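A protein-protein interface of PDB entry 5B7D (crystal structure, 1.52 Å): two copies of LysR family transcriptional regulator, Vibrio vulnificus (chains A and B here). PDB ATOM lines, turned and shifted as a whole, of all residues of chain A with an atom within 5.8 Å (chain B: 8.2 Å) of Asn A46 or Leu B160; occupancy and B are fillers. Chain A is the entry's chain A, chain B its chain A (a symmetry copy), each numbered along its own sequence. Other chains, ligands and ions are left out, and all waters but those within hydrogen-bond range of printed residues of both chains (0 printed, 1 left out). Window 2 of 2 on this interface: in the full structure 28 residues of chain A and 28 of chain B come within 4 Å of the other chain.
OG1 of Thr B163 sits at hydrogen-bond distance from O of Phe B117 (2.6 Å).
N of Phe B144 lies within hydrogen-bond range of OD1 of Asn B142 (2.8 Å).
The backbone carbonyl oxygen of Met B155 sits at hydrogen-bond distance from the backbone NH of Leu B160 (3.3 Å).
O of Leu A18 is in hydrogen-bond range of N of Leu A48.
N of Asn A46 is in hydrogen-bond range of O of Gly A16.
N of Phe B117 sits at hydrogen-bond distance from O of Thr B162 (3.0 Å).
No position is printed for both chains.
Asn A46 touches just these residues of chain B: Asn B158 and Leu B160.
Of the printed residues of chain A, Leu B160 touches Asn A46, Leu A47 and Leu A48.
Of the printed residues of chain A, Met B155 touches Leu A47 and Leu A48.
Printed residues of chain B within 4 Å of Leu A48: Phe B117, Phe B144, Met B155 and Leu B160.
Of the printed residues of chain B, Leu A47 touches Met B155, Asn B158 and Leu B160.
The nearest residue of chain B that does not touch Asn A46 is Gly B159 (6.1 Å).
The nearest printed residue of chain A that does not touch Leu B160 is Leu A45 (5.5 Å).
The nearest printed residue of chain B that does not touch Leu A47 is Gln B154 (5.8 Å).
Hydrophobic or aromatic side chains of chain B within 4 Å of the printed part of chain A: Phe B117, Phe B144, Met B155 and Leu B160.
Of the 13 printed residues of chain A, 5 touch a printed residue of chain B.
Hydrophobic or aromatic side chains of chain A that line the printed part of chain B: Ile A38, Leu A47 and Leu A48.
The backbone NH (N) of Leu A47 lies close to the side-chain amide nitrogen (ND2) of Asn B158 (2.9 Å).
Ile A38 touches Asn B158 (CD1 to OD1, 3.6 Å).
Asn B158 touches Leu A45 (OD1 to O, 3.7 Å).
CA of Asn A46 touches ND2 of Asn B158 (3.6 Å).
Leu B160 touches Asn A46.
CG of Met B155 touches O of Leu A47, 3.6 Å away.
Leu B160 touches Leu A47 (CD1 to O, 3.5 Å).
CE1 of Phe B117 touches CD2 of Leu A48 (3.95 Å).
Phe B144 touches Leu A48.
CA of Leu A48 touches SD of Met B155, 3.8 Å away.
Leu A48 touches Leu B160 (CD2 to CD1, 3.99 Å).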
ATOM      1  N   GLN A  15      -0.611 -30.119  12.869  1.00  0.00           N
ATOM      2  CA  GLN A  15       0.404 -29.379  13.587  1.00  0.00           C
ATOM      3  C   GLN A  15       1.427 -28.857  12.591  1.00  0.00           C
ATOM      4  O   GLN A  15       1.518 -29.314  11.449  1.00  0.00           O
ATOM      5  CB  GLN A  15       1.085 -30.248  14.655  1.00  0.00           C
ATOM      6  CG  GLN A  15       0.129 -30.846  15.675  1.00  0.00           C
ATOM      7  CD  GLN A  15       0.819 -31.246  16.972  1.00  0.00           C
ATOM      8  OE1 GLN A  15       1.669 -30.518  17.491  1.00  0.00           O
ATOM      9  NE2 GLN A  15       0.451 -32.408  17.503  1.00  0.00           N
ATOM     10  N   GLY A  16       2.199 -27.892  13.039  1.00  0.00           N
ATOM     11  CA  GLY A  16       3.258 -27.373  12.224  1.00  0.00           C
ATOM     12  C   GLY A  16       2.768 -26.215  11.378  1.00  0.00           C
ATOM     13  O   GLY A  16       1.754 -25.569  11.655  1.00  0.00           O
ATOM     14  N   GLN A  17       3.495 -25.990  10.297  1.00  0.00           N
ATOM     15  CA  GLN A  17       3.338 -24.817   9.449  1.00  0.00           C
ATOM     16  C   GLN A  17       2.701 -25.209   8.125  1.00  0.00           C
ATOM     17  O   GLN A  17       2.998 -26.271   7.578  1.00  0.00           O
ATOM     18  CB  GLN A  17       4.702 -24.190   9.206  1.00  0.00           C
ATOM     19  CG  GLN A  17       4.704 -22.816   8.634  1.00  0.00           C
ATOM     20  CD  GLN A  17       6.122 -22.285   8.542  1.00  0.00           C
ATOM     21  OE1 GLN A  17       6.591 -21.568   9.430  1.00  0.00           O
ATOM     22  NE2 GLN A  17       6.817 -22.645   7.466  1.00  0.00           N
ATOM     23  N   LEU A  18       1.808 -24.360   7.623  1.00  0.00           N
ATOM     24  CA  LEU A  18       1.204 -24.532   6.308  1.00  0.00           C
ATOM     25  C   LEU A  18       1.258 -23.196   5.586  1.00  0.00           C
ATOM     26  O   LEU A  18       0.943 -22.168   6.190  1.00  0.00           O
ATOM     27  CB  LEU A  18      -0.236 -25.001   6.439  1.00  0.00           C
ATOM     28  CG  LEU A  18      -0.926 -25.714   5.296  1.00  0.00           C
ATOM     29  CD1 LEU A  18      -0.185 -26.998   4.957  1.00  0.00           C
ATOM     30  CD2 LEU A  18      -2.338 -26.011   5.746  1.00  0.00           C
ATOM     31  N   LYS A  19       1.668 -23.206   4.318  1.00  0.00           N
ATOM     32  CA  LYS A  19       1.627 -22.024   3.460  1.00  0.00           C
ATOM     33  C   LYS A  19       0.397 -22.076   2.564  1.00  0.00           C
ATOM     34  O   LYS A  19       0.287 -22.953   1.698  1.00  0.00           O
ATOM     35  CB  LYS A  19       2.896 -21.923   2.609  1.00  0.00           C
ATOM     36  CG  LYS A  19       4.152 -21.709   3.464  1.00  0.00           C
ATOM     37  CD  LYS A  19       5.383 -21.527   2.586  1.00  0.00           C
ATOM     38  CE  LYS A  19       6.584 -21.123   3.381  1.00  0.00           C
ATOM     39  NZ  LYS A  19       7.839 -21.310   2.578  1.00  0.00           N
ATOM     40  N   ILE A  38      -9.374 -22.314  13.398  1.00  0.00           N
ATOM     41  CA  ILE A  38      -8.197 -23.165  13.615  1.00  0.00           C
ATOM     42  C   ILE A  38      -7.465 -22.778  14.895  1.00  0.00           C
ATOM     43  O   ILE A  38      -6.856 -23.641  15.539  1.00  0.00           O
ATOM     44  CB  ILE A  38      -7.237 -23.181  12.406  1.00  0.00           C
ATOM     45  CG1 ILE A  38      -6.538 -21.845  12.211  1.00  0.00           C
ATOM     46  CG2 ILE A  38      -7.933 -23.696  11.125  1.00  0.00           C
ATOM     47  CD1 ILE A  38      -5.335 -21.959  11.240  1.00  0.00           C
ATOM     48  N   PHE A  42      -7.310 -26.355  16.075  1.00  0.00           N
ATOM     49  CA  PHE A  42      -5.988 -26.866  15.710  1.00  0.00           C
ATOM     50  C   PHE A  42      -4.950 -25.845  16.153  1.00  0.00           C
ATOM     51  O   PHE A  42      -4.300 -25.189  15.327  1.00  0.00           O
ATOM     52  CB  PHE A  42      -5.906 -27.156  14.211  1.00  0.00           C
ATOM     53  CG  PHE A  42      -7.005 -28.046  13.720  1.00  0.00           C
ATOM     54  CD1 PHE A  42      -7.017 -29.392  14.051  1.00  0.00           C
ATOM     55  CD2 PHE A  42      -8.045 -27.540  12.966  1.00  0.00           C
ATOM     56  CE1 PHE A  42      -8.032 -30.229  13.608  1.00  0.00           C
ATOM     57  CE2 PHE A  42      -9.067 -28.369  12.521  1.00  0.00           C
ATOM     58  CZ  PHE A  42      -9.060 -29.716  12.846  1.00  0.00           C
ATOM     59  N   PRO A  43      -4.768 -25.692  17.469  1.00  0.00           N
ATOM     60  CA  PRO A  43      -3.963 -24.578  17.980  1.00  0.00           C
ATOM     61  C   PRO A  43      -2.492 -24.648  17.619  1.00  0.00           C
ATOM     62  O   PRO A  43      -1.805 -23.629  17.769  1.00  0.00           O
ATOM     63  CB  PRO A  43      -4.172 -24.660  19.502  1.00  0.00           C
ATOM     64  CG  PRO A  43      -4.619 -26.065  19.756  1.00  0.00           C
ATOM     65  CD  PRO A  43      -5.395 -26.472  18.549  1.00  0.00           C
ATOM     66  N   GLN A  44      -1.980 -25.792  17.148  1.00  0.00           N
ATOM     67  CA  GLN A  44      -0.580 -25.894  16.754  1.00  0.00           C
ATOM     68  C   GLN A  44      -0.369 -25.742  15.251  1.00  0.00           C
ATOM     69  O   GLN A  44       0.745 -25.962  14.772  1.00  0.00           O
ATOM     70  CB  GLN A  44       0.004 -27.219  17.230  1.00  0.00           C
ATOM     71  CG  GLN A  44       0.429 -27.196  18.682  1.00  0.00           C
ATOM     72  CD  GLN A  44      -0.750 -27.248  19.616  1.00  0.00           C
ATOM     73  OE1 GLN A  44      -1.587 -28.148  19.524  1.00  0.00           O
ATOM     74  NE2 GLN A  44      -0.831 -26.280  20.526  1.00  0.00           N
ATOM     75  N   LEU A  45      -1.404 -25.369  14.504  1.00  0.00           N
ATOM     76  CA  LEU A  45      -1.287 -25.107  13.073  1.00  0.00           C
ATOM     77  C   LEU A  45      -0.995 -23.629  12.846  1.00  0.00           C
ATOM     78  O   LEU A  45      -1.818 -22.770  13.187  1.00  0.00           O
ATOM     79  CB  LEU A  45      -2.568 -25.507  12.342  1.00  0.00           C
ATOM     80  CG  LEU A  45      -2.504 -25.503  10.807  1.00  0.00           C
ATOM     81  CD1 LEU A  45      -1.352 -26.390  10.301  1.00  0.00           C
ATOM     82  CD2 LEU A  45      -3.833 -25.957  10.244  1.00  0.00           C
ATOM     83  N   ASN A  46       0.183 -23.338  12.308  1.00  0.00           N
ATOM     84  CA  ASN A  46       0.574 -21.979  11.953  1.00  0.00           C
ATOM     85  C   ASN A  46       0.302 -21.792  10.470  1.00  0.00           C
ATOM     86  O   ASN A  46       0.855 -22.523   9.640  1.00  0.00           O
ATOM     87  CB  ASN A  46       2.052 -21.729  12.271  1.00  0.00           C
ATOM     88  CG  ASN A  46       2.321 -21.627  13.754  1.00  0.00           C
ATOM     89  OD1 ASN A  46       1.397 -21.653  14.573  1.00  0.00           O
ATOM     90  ND2 ASN A  46       3.586 -21.475  14.113  1.00  0.00           N
ATOM     91  N   LEU A  47      -0.556 -20.825  10.133  1.00  0.00           N
ATOM     92  CA  LEU A  47      -0.956 -20.574   8.751  1.00  0.00           C
ATOM     93  C   LEU A  47      -0.219 -19.350   8.225  1.00  0.00           C
ATOM     94  O   LEU A  47      -0.558 -18.225   8.578  1.00  0.00           O
ATOM     95  CB  LEU A  47      -2.463 -20.354   8.655  1.00  0.00           C
ATOM     96  CG  LEU A  47      -3.465 -21.381   8.161  1.00  0.00           C
ATOM     97  CD1 LEU A  47      -4.741 -20.604   7.830  1.00  0.00           C
ATOM     98  CD2 LEU A  47      -2.960 -22.163   6.955  1.00  0.00           C
ATOM     99  N   LEU A  48       0.783 -19.573   7.371  1.00  0.00           N
ATOM    100  CA  LEU A  48       1.432 -18.503   6.623  1.00  0.00           C
ATOM    101  C   LEU A  48       0.597 -18.253   5.377  1.00  0.00           C
ATOM    102  O   LEU A  48       0.194 -19.205   4.701  1.00  0.00           O
ATOM    103  CB  LEU A  48       2.860 -18.890   6.240  1.00  0.00           C
ATOM    104  CG  LEU A  48       3.790 -19.130   7.433  1.00  0.00           C
ATOM    105  CD1 LEU A  48       5.119 -19.614   6.894  1.00  0.00           C
ATOM    106  CD2 LEU A  48       4.011 -17.820   8.201  1.00  0.00           C
ATOM    107  N   ILE B  94      -1.383  -7.389  18.322  1.00  0.00           N
ATOM    108  CA  ILE B  94      -1.053  -8.759  18.682  1.00  0.00           C
ATOM    109  C   ILE B  94      -2.363  -9.476  18.961  1.00  0.00           C
ATOM    110  O   ILE B  94      -3.388  -8.858  19.264  1.00  0.00           O
ATOM    111  CB  ILE B  94      -0.143  -8.836  19.922  1.00  0.00           C
ATOM    112  CG1 ILE B  94      -0.868  -8.267  21.140  1.00  0.00           C
ATOM    113  CG2 ILE B  94       1.144  -8.082  19.688  1.00  0.00           C
ATOM    114  CD1 ILE B  94      -0.024  -8.273  22.379  1.00  0.00           C
ATOM    115  N   SER B  95      -2.326 -10.796  18.870  1.00  0.00           N
ATOM    116  CA  SER B  95      -3.516 -11.544  19.251  1.00  0.00           C
ATOM    117  C   SER B  95      -3.701 -11.505  20.762  1.00  0.00           C
ATOM    118  O   SER B  95      -2.739 -11.441  21.536  1.00  0.00           O
ATOM    119  CB  SER B  95      -3.426 -12.989  18.767  1.00  0.00           C
ATOM    120  OG  SER B  95      -2.459 -13.665  19.542  1.00  0.00           O
ATOM    121  N   GLN B  98      -1.715 -14.103  22.508  1.00  0.00           N
ATOM    122  CA  GLN B  98      -0.274 -13.896  22.650  1.00  0.00           C
ATOM    123  C   GLN B  98       0.030 -12.638  23.430  1.00  0.00           C
ATOM    124  O   GLN B  98       1.201 -12.270  23.561  1.00  0.00           O
ATOM    125  CB  GLN B  98       0.421 -13.814  21.279  1.00  0.00           C
ATOM    126  CG  GLN B  98       0.291 -15.051  20.391  1.00  0.00           C
ATOM    127  CD  GLN B  98       1.098 -16.247  20.895  1.00  0.00           C
ATOM    128  OE1 GLN B  98       2.275 -16.122  21.237  1.00  0.00           O
ATOM    129  NE2 GLN B  98       0.461 -17.413  20.934  1.00  0.00           N
ATOM    130  N   ILE B 102       4.000 -11.057  25.197  1.00  0.00           N
ATOM    131  CA  ILE B 102       4.623  -9.849  24.674  1.00  0.00           C
ATOM    132  C   ILE B 102       4.284  -8.699  25.618  1.00  0.00           C
ATOM    133  O   ILE B 102       3.105  -8.412  25.856  1.00  0.00           O
ATOM    134  CB  ILE B 102       4.172  -9.556  23.232  1.00  0.00           C
ATOM    135  CG1 ILE B 102       5.020 -10.386  22.264  1.00  0.00           C
ATOM    136  CG2 ILE B 102       4.299  -8.087  22.912  1.00  0.00           C
ATOM    137  CD1 ILE B 102       4.353 -10.730  20.962  1.00  0.00           C
ATOM    138  N   PRO B 112      10.688 -11.772  20.471  1.00  0.00           N
ATOM    139  CA  PRO B 112      11.423 -12.877  19.858  1.00  0.00           C
ATOM    140  C   PRO B 112      11.957 -12.494  18.487  1.00  0.00           C
ATOM    141  O   PRO B 112      11.387 -11.662  17.783  1.00  0.00           O
ATOM    142  CB  PRO B 112      10.375 -13.994  19.750  1.00  0.00           C
ATOM    143  CG  PRO B 112       9.322 -13.641  20.696  1.00  0.00           C
ATOM    144  CD  PRO B 112       9.286 -12.144  20.738  1.00  0.00           C
ATOM    145  N   ASP B 113      13.069 -13.121  18.109  1.00  0.00           N
ATOM    146  CA  ASP B 113      13.534 -13.010  16.732  1.00  0.00           C
ATOM    147  C   ASP B 113      12.440 -13.485  15.785  1.00  0.00           C
ATOM    148  O   ASP B 113      11.661 -14.385  16.116  1.00  0.00           O
ATOM    149  CB  ASP B 113      14.798 -13.851  16.525  1.00  0.00           C
ATOM    150  CG  ASP B 113      16.025 -13.244  17.171  1.00  0.00           C
ATOM    151  OD1 ASP B 113      15.985 -12.073  17.604  1.00  0.00           O
ATOM    152  OD2 ASP B 113      17.053 -13.947  17.222  1.00  0.00           O
ATOM    153  N   GLU B 114      12.362 -12.835  14.615  1.00  0.00           N
ATOM    154  CA  GLU B 114      11.395 -13.168  13.556  1.00  0.00           C
ATOM    155  C   GLU B 114       9.940 -13.062  14.007  1.00  0.00           C
ATOM    156  O   GLU B 114       9.065 -13.734  13.457  1.00  0.00           O
ATOM    157  CB  GLU B 114      11.648 -14.559  12.958  1.00  0.00           C
ATOM    158  CG  GLU B 114      13.103 -14.766  12.536  1.00  0.00           C
ATOM    159  CD  GLU B 114      13.332 -16.052  11.752  1.00  0.00           C
ATOM    160  OE1 GLU B 114      14.438 -16.211  11.192  1.00  0.00           O
ATOM    161  OE2 GLU B 114      12.407 -16.885  11.659  1.00  0.00           O
ATOM    162  N   SER B 115       9.634 -12.199  14.979  1.00  0.00           N
ATOM    163  CA  SER B 115       8.261 -12.067  15.437  1.00  0.00           C
ATOM    164  C   SER B 115       7.497 -10.936  14.744  1.00  0.00           C
ATOM    165  O   SER B 115       6.270 -10.871  14.893  1.00  0.00           O
ATOM    166  CB  SER B 115       8.234 -11.862  16.967  1.00  0.00           C
ATOM    167  OG  SER B 115       8.949 -10.696  17.342  1.00  0.00           O
ATOM    168  N   VAL B 116       8.162 -10.071  13.980  1.00  0.00           N
ATOM    169  CA  VAL B 116       7.503  -8.935  13.324  1.00  0.00           C
ATOM    170  C   VAL B 116       7.282  -9.276  11.852  1.00  0.00           C
ATOM    171  O   VAL B 116       8.241  -9.431  11.081  1.00  0.00           O
ATOM    172  CB  VAL B 116       8.324  -7.641  13.464  1.00  0.00           C
ATOM    173  CG1 VAL B 116       7.607  -6.481  12.763  1.00  0.00           C
ATOM    174  CG2 VAL B 116       8.586  -7.329  14.923  1.00  0.00           C
ATOM    175  N   PHE B 117       6.023  -9.398  11.453  1.00  0.00           N
ATOM    176  CA  PHE B 117       5.682  -9.664  10.062  1.00  0.00           C
ATOM    177  C   PHE B 117       5.474  -8.343   9.335  1.00  0.00           C
ATOM    178  O   PHE B 117       4.965  -7.381   9.919  1.00  0.00           O
ATOM    179  CB  PHE B 117       4.415 -10.520   9.982  1.00  0.00           C
ATOM    180  CG  PHE B 117       4.639 -11.965  10.324  1.00  0.00           C
ATOM    181  CD1 PHE B 117       4.746 -12.920   9.311  1.00  0.00           C
ATOM    182  CD2 PHE B 117       4.741 -12.374  11.653  1.00  0.00           C
ATOM    183  CE1 PHE B 117       4.955 -14.256   9.627  1.00  0.00           C
ATOM    184  CE2 PHE B 117       4.952 -13.720  11.989  1.00  0.00           C
ATOM    185  CZ  PHE B 117       5.064 -14.661  10.973  1.00  0.00           C
ATOM    186  N   ASN B 142      10.197 -11.315  10.559  1.00  0.00           N
ATOM    187  CA  ASN B 142      10.016 -12.671  10.060  1.00  0.00           C
ATOM    188  C   ASN B 142      10.394 -12.731   8.580  1.00  0.00           C
ATOM    189  O   ASN B 142      10.032 -11.825   7.815  1.00  0.00           O
ATOM    190  CB  ASN B 142       8.566 -13.118  10.230  1.00  0.00           C
ATOM    191  CG  ASN B 142       8.405 -14.606  10.028  1.00  0.00           C
ATOM    192  OD1 ASN B 142       8.386 -15.074   8.884  1.00  0.00           O
ATOM    193  ND2 ASN B 142       8.320 -15.374  11.136  1.00  0.00           N
ATOM    194  N   PHE B 144       9.198 -14.514   6.237  1.00  0.00           N
ATOM    195  CA  PHE B 144       8.067 -14.734   5.342  1.00  0.00           C
ATOM    196  C   PHE B 144       7.319 -13.415   5.183  1.00  0.00           C
ATOM    197  O   PHE B 144       6.719 -12.917   6.144  1.00  0.00           O
ATOM    198  CB  PHE B 144       7.145 -15.823   5.875  1.00  0.00           C
ATOM    199  CG  PHE B 144       5.988 -16.118   4.953  1.00  0.00           C
ATOM    200  CD1 PHE B 144       4.760 -15.471   5.123  1.00  0.00           C
ATOM    201  CD2 PHE B 144       6.137 -17.017   3.900  1.00  0.00           C
ATOM    202  CE1 PHE B 144       3.694 -15.741   4.266  1.00  0.00           C
ATOM    203  CE2 PHE B 144       5.077 -17.275   3.039  1.00  0.00           C
ATOM    204  CZ  PHE B 144       3.859 -16.636   3.229  1.00  0.00           C
ATOM    205  N   THR B 151      -4.248 -10.249   4.913  1.00  0.00           N
ATOM    206  CA  THR B 151      -3.628 -11.528   5.279  1.00  0.00           C
ATOM    207  C   THR B 151      -2.498 -11.329   6.279  1.00  0.00           C
ATOM    208  O   THR B 151      -2.244 -12.215   7.099  1.00  0.00           O
ATOM    209  CB  THR B 151      -3.135 -12.286   4.035  1.00  0.00           C
ATOM    210  OG1 THR B 151      -2.221 -11.486   3.268  1.00  0.00           O
ATOM    211  CG2 THR B 151      -4.332 -12.700   3.136  1.00  0.00           C
ATOM    212  N   LEU B 152      -1.832 -10.170   6.263  1.00  0.00           N
ATOM    213  CA  LEU B 152      -0.889  -9.849   7.329  1.00  0.00           C
ATOM    214  C   LEU B 152      -1.583  -9.877   8.686  1.00  0.00           C
ATOM    215  O   LEU B 152      -1.100 -10.512   9.644  1.00  0.00           O
ATOM    216  CB  LEU B 152      -0.269  -8.476   7.046  1.00  0.00           C
ATOM    217  CG  LEU B 152       0.613  -7.867   8.136  1.00  0.00           C
ATOM    218  CD1 LEU B 152       1.766  -8.815   8.469  1.00  0.00           C
ATOM    219  CD2 LEU B 152       1.159  -6.524   7.669  1.00  0.00           C
ATOM    220  N   VAL B 153      -2.722  -9.197   8.789  1.00  0.00           N
ATOM    221  CA  VAL B 153      -3.427  -9.126  10.061  1.00  0.00           C
ATOM    222  C   VAL B 153      -3.939 -10.498  10.456  1.00  0.00           C
ATOM    223  O   VAL B 153      -3.931 -10.853  11.633  1.00  0.00           O
ATOM    224  CB  VAL B 153      -4.565  -8.093   9.973  1.00  0.00           C
ATOM    225  CG1 VAL B 153      -5.495  -8.199  11.198  1.00  0.00           C
ATOM    226  CG2 VAL B 153      -3.975  -6.678   9.899  1.00  0.00           C
ATOM    227  N   GLN B 154      -4.360 -11.307   9.478  1.00  0.00           N
ATOM    228  CA  GLN B 154      -4.835 -12.655   9.780  1.00  0.00           C
ATOM    229  C   GLN B 154      -3.716 -13.525  10.361  1.00  0.00           C
ATOM    230  O   GLN B 154      -3.961 -14.313  11.278  1.00  0.00           O
ATOM    231  CB  GLN B 154      -5.399 -13.286   8.511  1.00  0.00           C
ATOM    232  CG  GLN B 154      -6.822 -12.868   8.179  1.00  0.00           C
ATOM    233  CD  GLN B 154      -7.066 -12.787   6.666  1.00  0.00           C
ATOM    234  OE1 GLN B 154      -6.284 -13.302   5.875  1.00  0.00           O
ATOM    235  NE2 GLN B 154      -8.220 -12.243   6.284  1.00  0.00           N
ATOM    236  N   MET B 155      -2.486 -13.404   9.835  1.00  0.00           N
ATOM    237  CA  MET B 155      -1.365 -14.137  10.440  1.00  0.00           C
ATOM    238  C   MET B 155      -1.135 -13.695  11.881  1.00  0.00           C
ATOM    239  O   MET B 155      -0.885 -14.530  12.758  1.00  0.00           O
ATOM    240  CB  MET B 155      -0.099 -13.953   9.611  1.00  0.00           C
ATOM    241  CG  MET B 155      -0.169 -14.690   8.262  1.00  0.00           C
ATOM    242  SD  MET B 155       1.423 -14.744   7.428  1.00  0.00           S
ATOM    243  CE  MET B 155       1.579 -13.054   6.799  1.00  0.00           C
ATOM    244  N   VAL B 156      -1.220 -12.390  12.149  1.00  0.00           N
ATOM    245  CA  VAL B 156      -1.137 -11.921  13.532  1.00  0.00           C
ATOM    246  C   VAL B 156      -2.276 -12.514  14.359  1.00  0.00           C
ATOM    247  O   VAL B 156      -2.068 -12.945  15.501  1.00  0.00           O
ATOM    248  CB  VAL B 156      -1.135 -10.380  13.582  1.00  0.00           C
ATOM    249  CG1 VAL B 156      -1.213  -9.899  15.052  1.00  0.00           C
ATOM    250  CG2 VAL B 156       0.150  -9.816  12.959  1.00  0.00           C
ATOM    251  N   ALA B 157      -3.492 -12.551  13.797  1.00  0.00           N
ATOM    252  CA  ALA B 157      -4.627 -13.087  14.534  1.00  0.00           C
ATOM    253  C   ALA B 157      -4.448 -14.573  14.822  1.00  0.00           C
ATOM    254  O   ALA B 157      -4.987 -15.090  15.812  1.00  0.00           O
ATOM    255  CB  ALA B 157      -5.939 -12.839  13.771  1.00  0.00           C
ATOM    256  N   ASN B 158      -3.712 -15.279  13.965  1.00  0.00           N
ATOM    257  CA  ASN B 158      -3.363 -16.682  14.174  1.00  0.00           C
ATOM    258  C   ASN B 158      -2.308 -16.868  15.265  1.00  0.00           C
ATOM    259  O   ASN B 158      -2.001 -18.024  15.599  1.00  0.00           O
ATOM    260  CB  ASN B 158      -2.875 -17.240  12.835  1.00  0.00           C
ATOM    261  CG  ASN B 158      -2.730 -18.760  12.808  1.00  0.00           C
ATOM    262  OD1 ASN B 158      -3.575 -19.537  13.295  1.00  0.00           O
ATOM    263  ND2 ASN B 158      -1.662 -19.184  12.188  1.00  0.00           N
ATOM    264  N   GLY B 159      -1.763 -15.786  15.834  1.00  0.00           N
ATOM    265  CA  GLY B 159      -0.815 -15.875  16.938  1.00  0.00           C
ATOM    266  C   GLY B 159       0.640 -15.880  16.527  1.00  0.00           C
ATOM    267  O   GLY B 159       1.506 -16.172  17.367  1.00  0.00           O
ATOM    268  N   LEU B 160       0.950 -15.533  15.276  1.00  0.00           N
ATOM    269  CA  LEU B 160       2.296 -15.779  14.770  1.00  0.00           C
ATOM    270  C   LEU B 160       3.285 -14.679  15.141  1.00  0.00           C
ATOM    271  O   LEU B 160       4.493 -14.917  15.090  1.00  0.00           O
ATOM    272  CB  LEU B 160       2.267 -15.960  13.245  1.00  0.00           C
ATOM    273  CG  LEU B 160       1.308 -17.054  12.774  1.00  0.00           C
ATOM    274  CD1 LEU B 160       1.527 -17.311  11.278  1.00  0.00           C
ATOM    275  CD2 LEU B 160       1.490 -18.356  13.584  1.00  0.00           C
ATOM    276  N   GLY B 161       2.808 -13.501  15.534  1.00  0.00           N
ATOM    277  CA  GLY B 161       3.706 -12.413  15.862  1.00  0.00           C
ATOM    278  C   GLY B 161       2.965 -11.096  15.921  1.00  0.00           C
ATOM    279  O   GLY B 161       1.815 -11.042  16.359  1.00  0.00           O
ATOM    280  N   THR B 162       3.617 -10.012  15.510  1.00  0.00           N
ATOM    281  CA  THR B 162       3.030  -8.687  15.638  1.00  0.00           C
ATOM    282  C   THR B 162       3.279  -7.940  14.333  1.00  0.00           C
ATOM    283  O   THR B 162       4.048  -8.391  13.476  1.00  0.00           O
ATOM    284  CB  THR B 162       3.622  -7.964  16.860  1.00  0.00           C
ATOM    285  OG1 THR B 162       2.958  -6.706  17.068  1.00  0.00           O
ATOM    286  CG2 THR B 162       5.135  -7.744  16.701  1.00  0.00           C
ATOM    287  N   THR B 163       2.593  -6.815  14.149  1.00  0.00           N
ATOM    288  CA  THR B 163       2.890  -5.984  12.985  1.00  0.00           C
ATOM    289  C   THR B 163       2.390  -4.577  13.256  1.00  0.00           C
ATOM    290  O   THR B 163       1.714  -4.327  14.250  1.00  0.00           O
ATOM    291  CB  THR B 163       2.248  -6.539  11.706  1.00  0.00           C
ATOM    292  OG1 THR B 163       2.920  -5.968  10.580  1.00  0.00           O
ATOM    293  CG2 THR B 163       0.757  -6.203  11.642  1.00  0.00           C
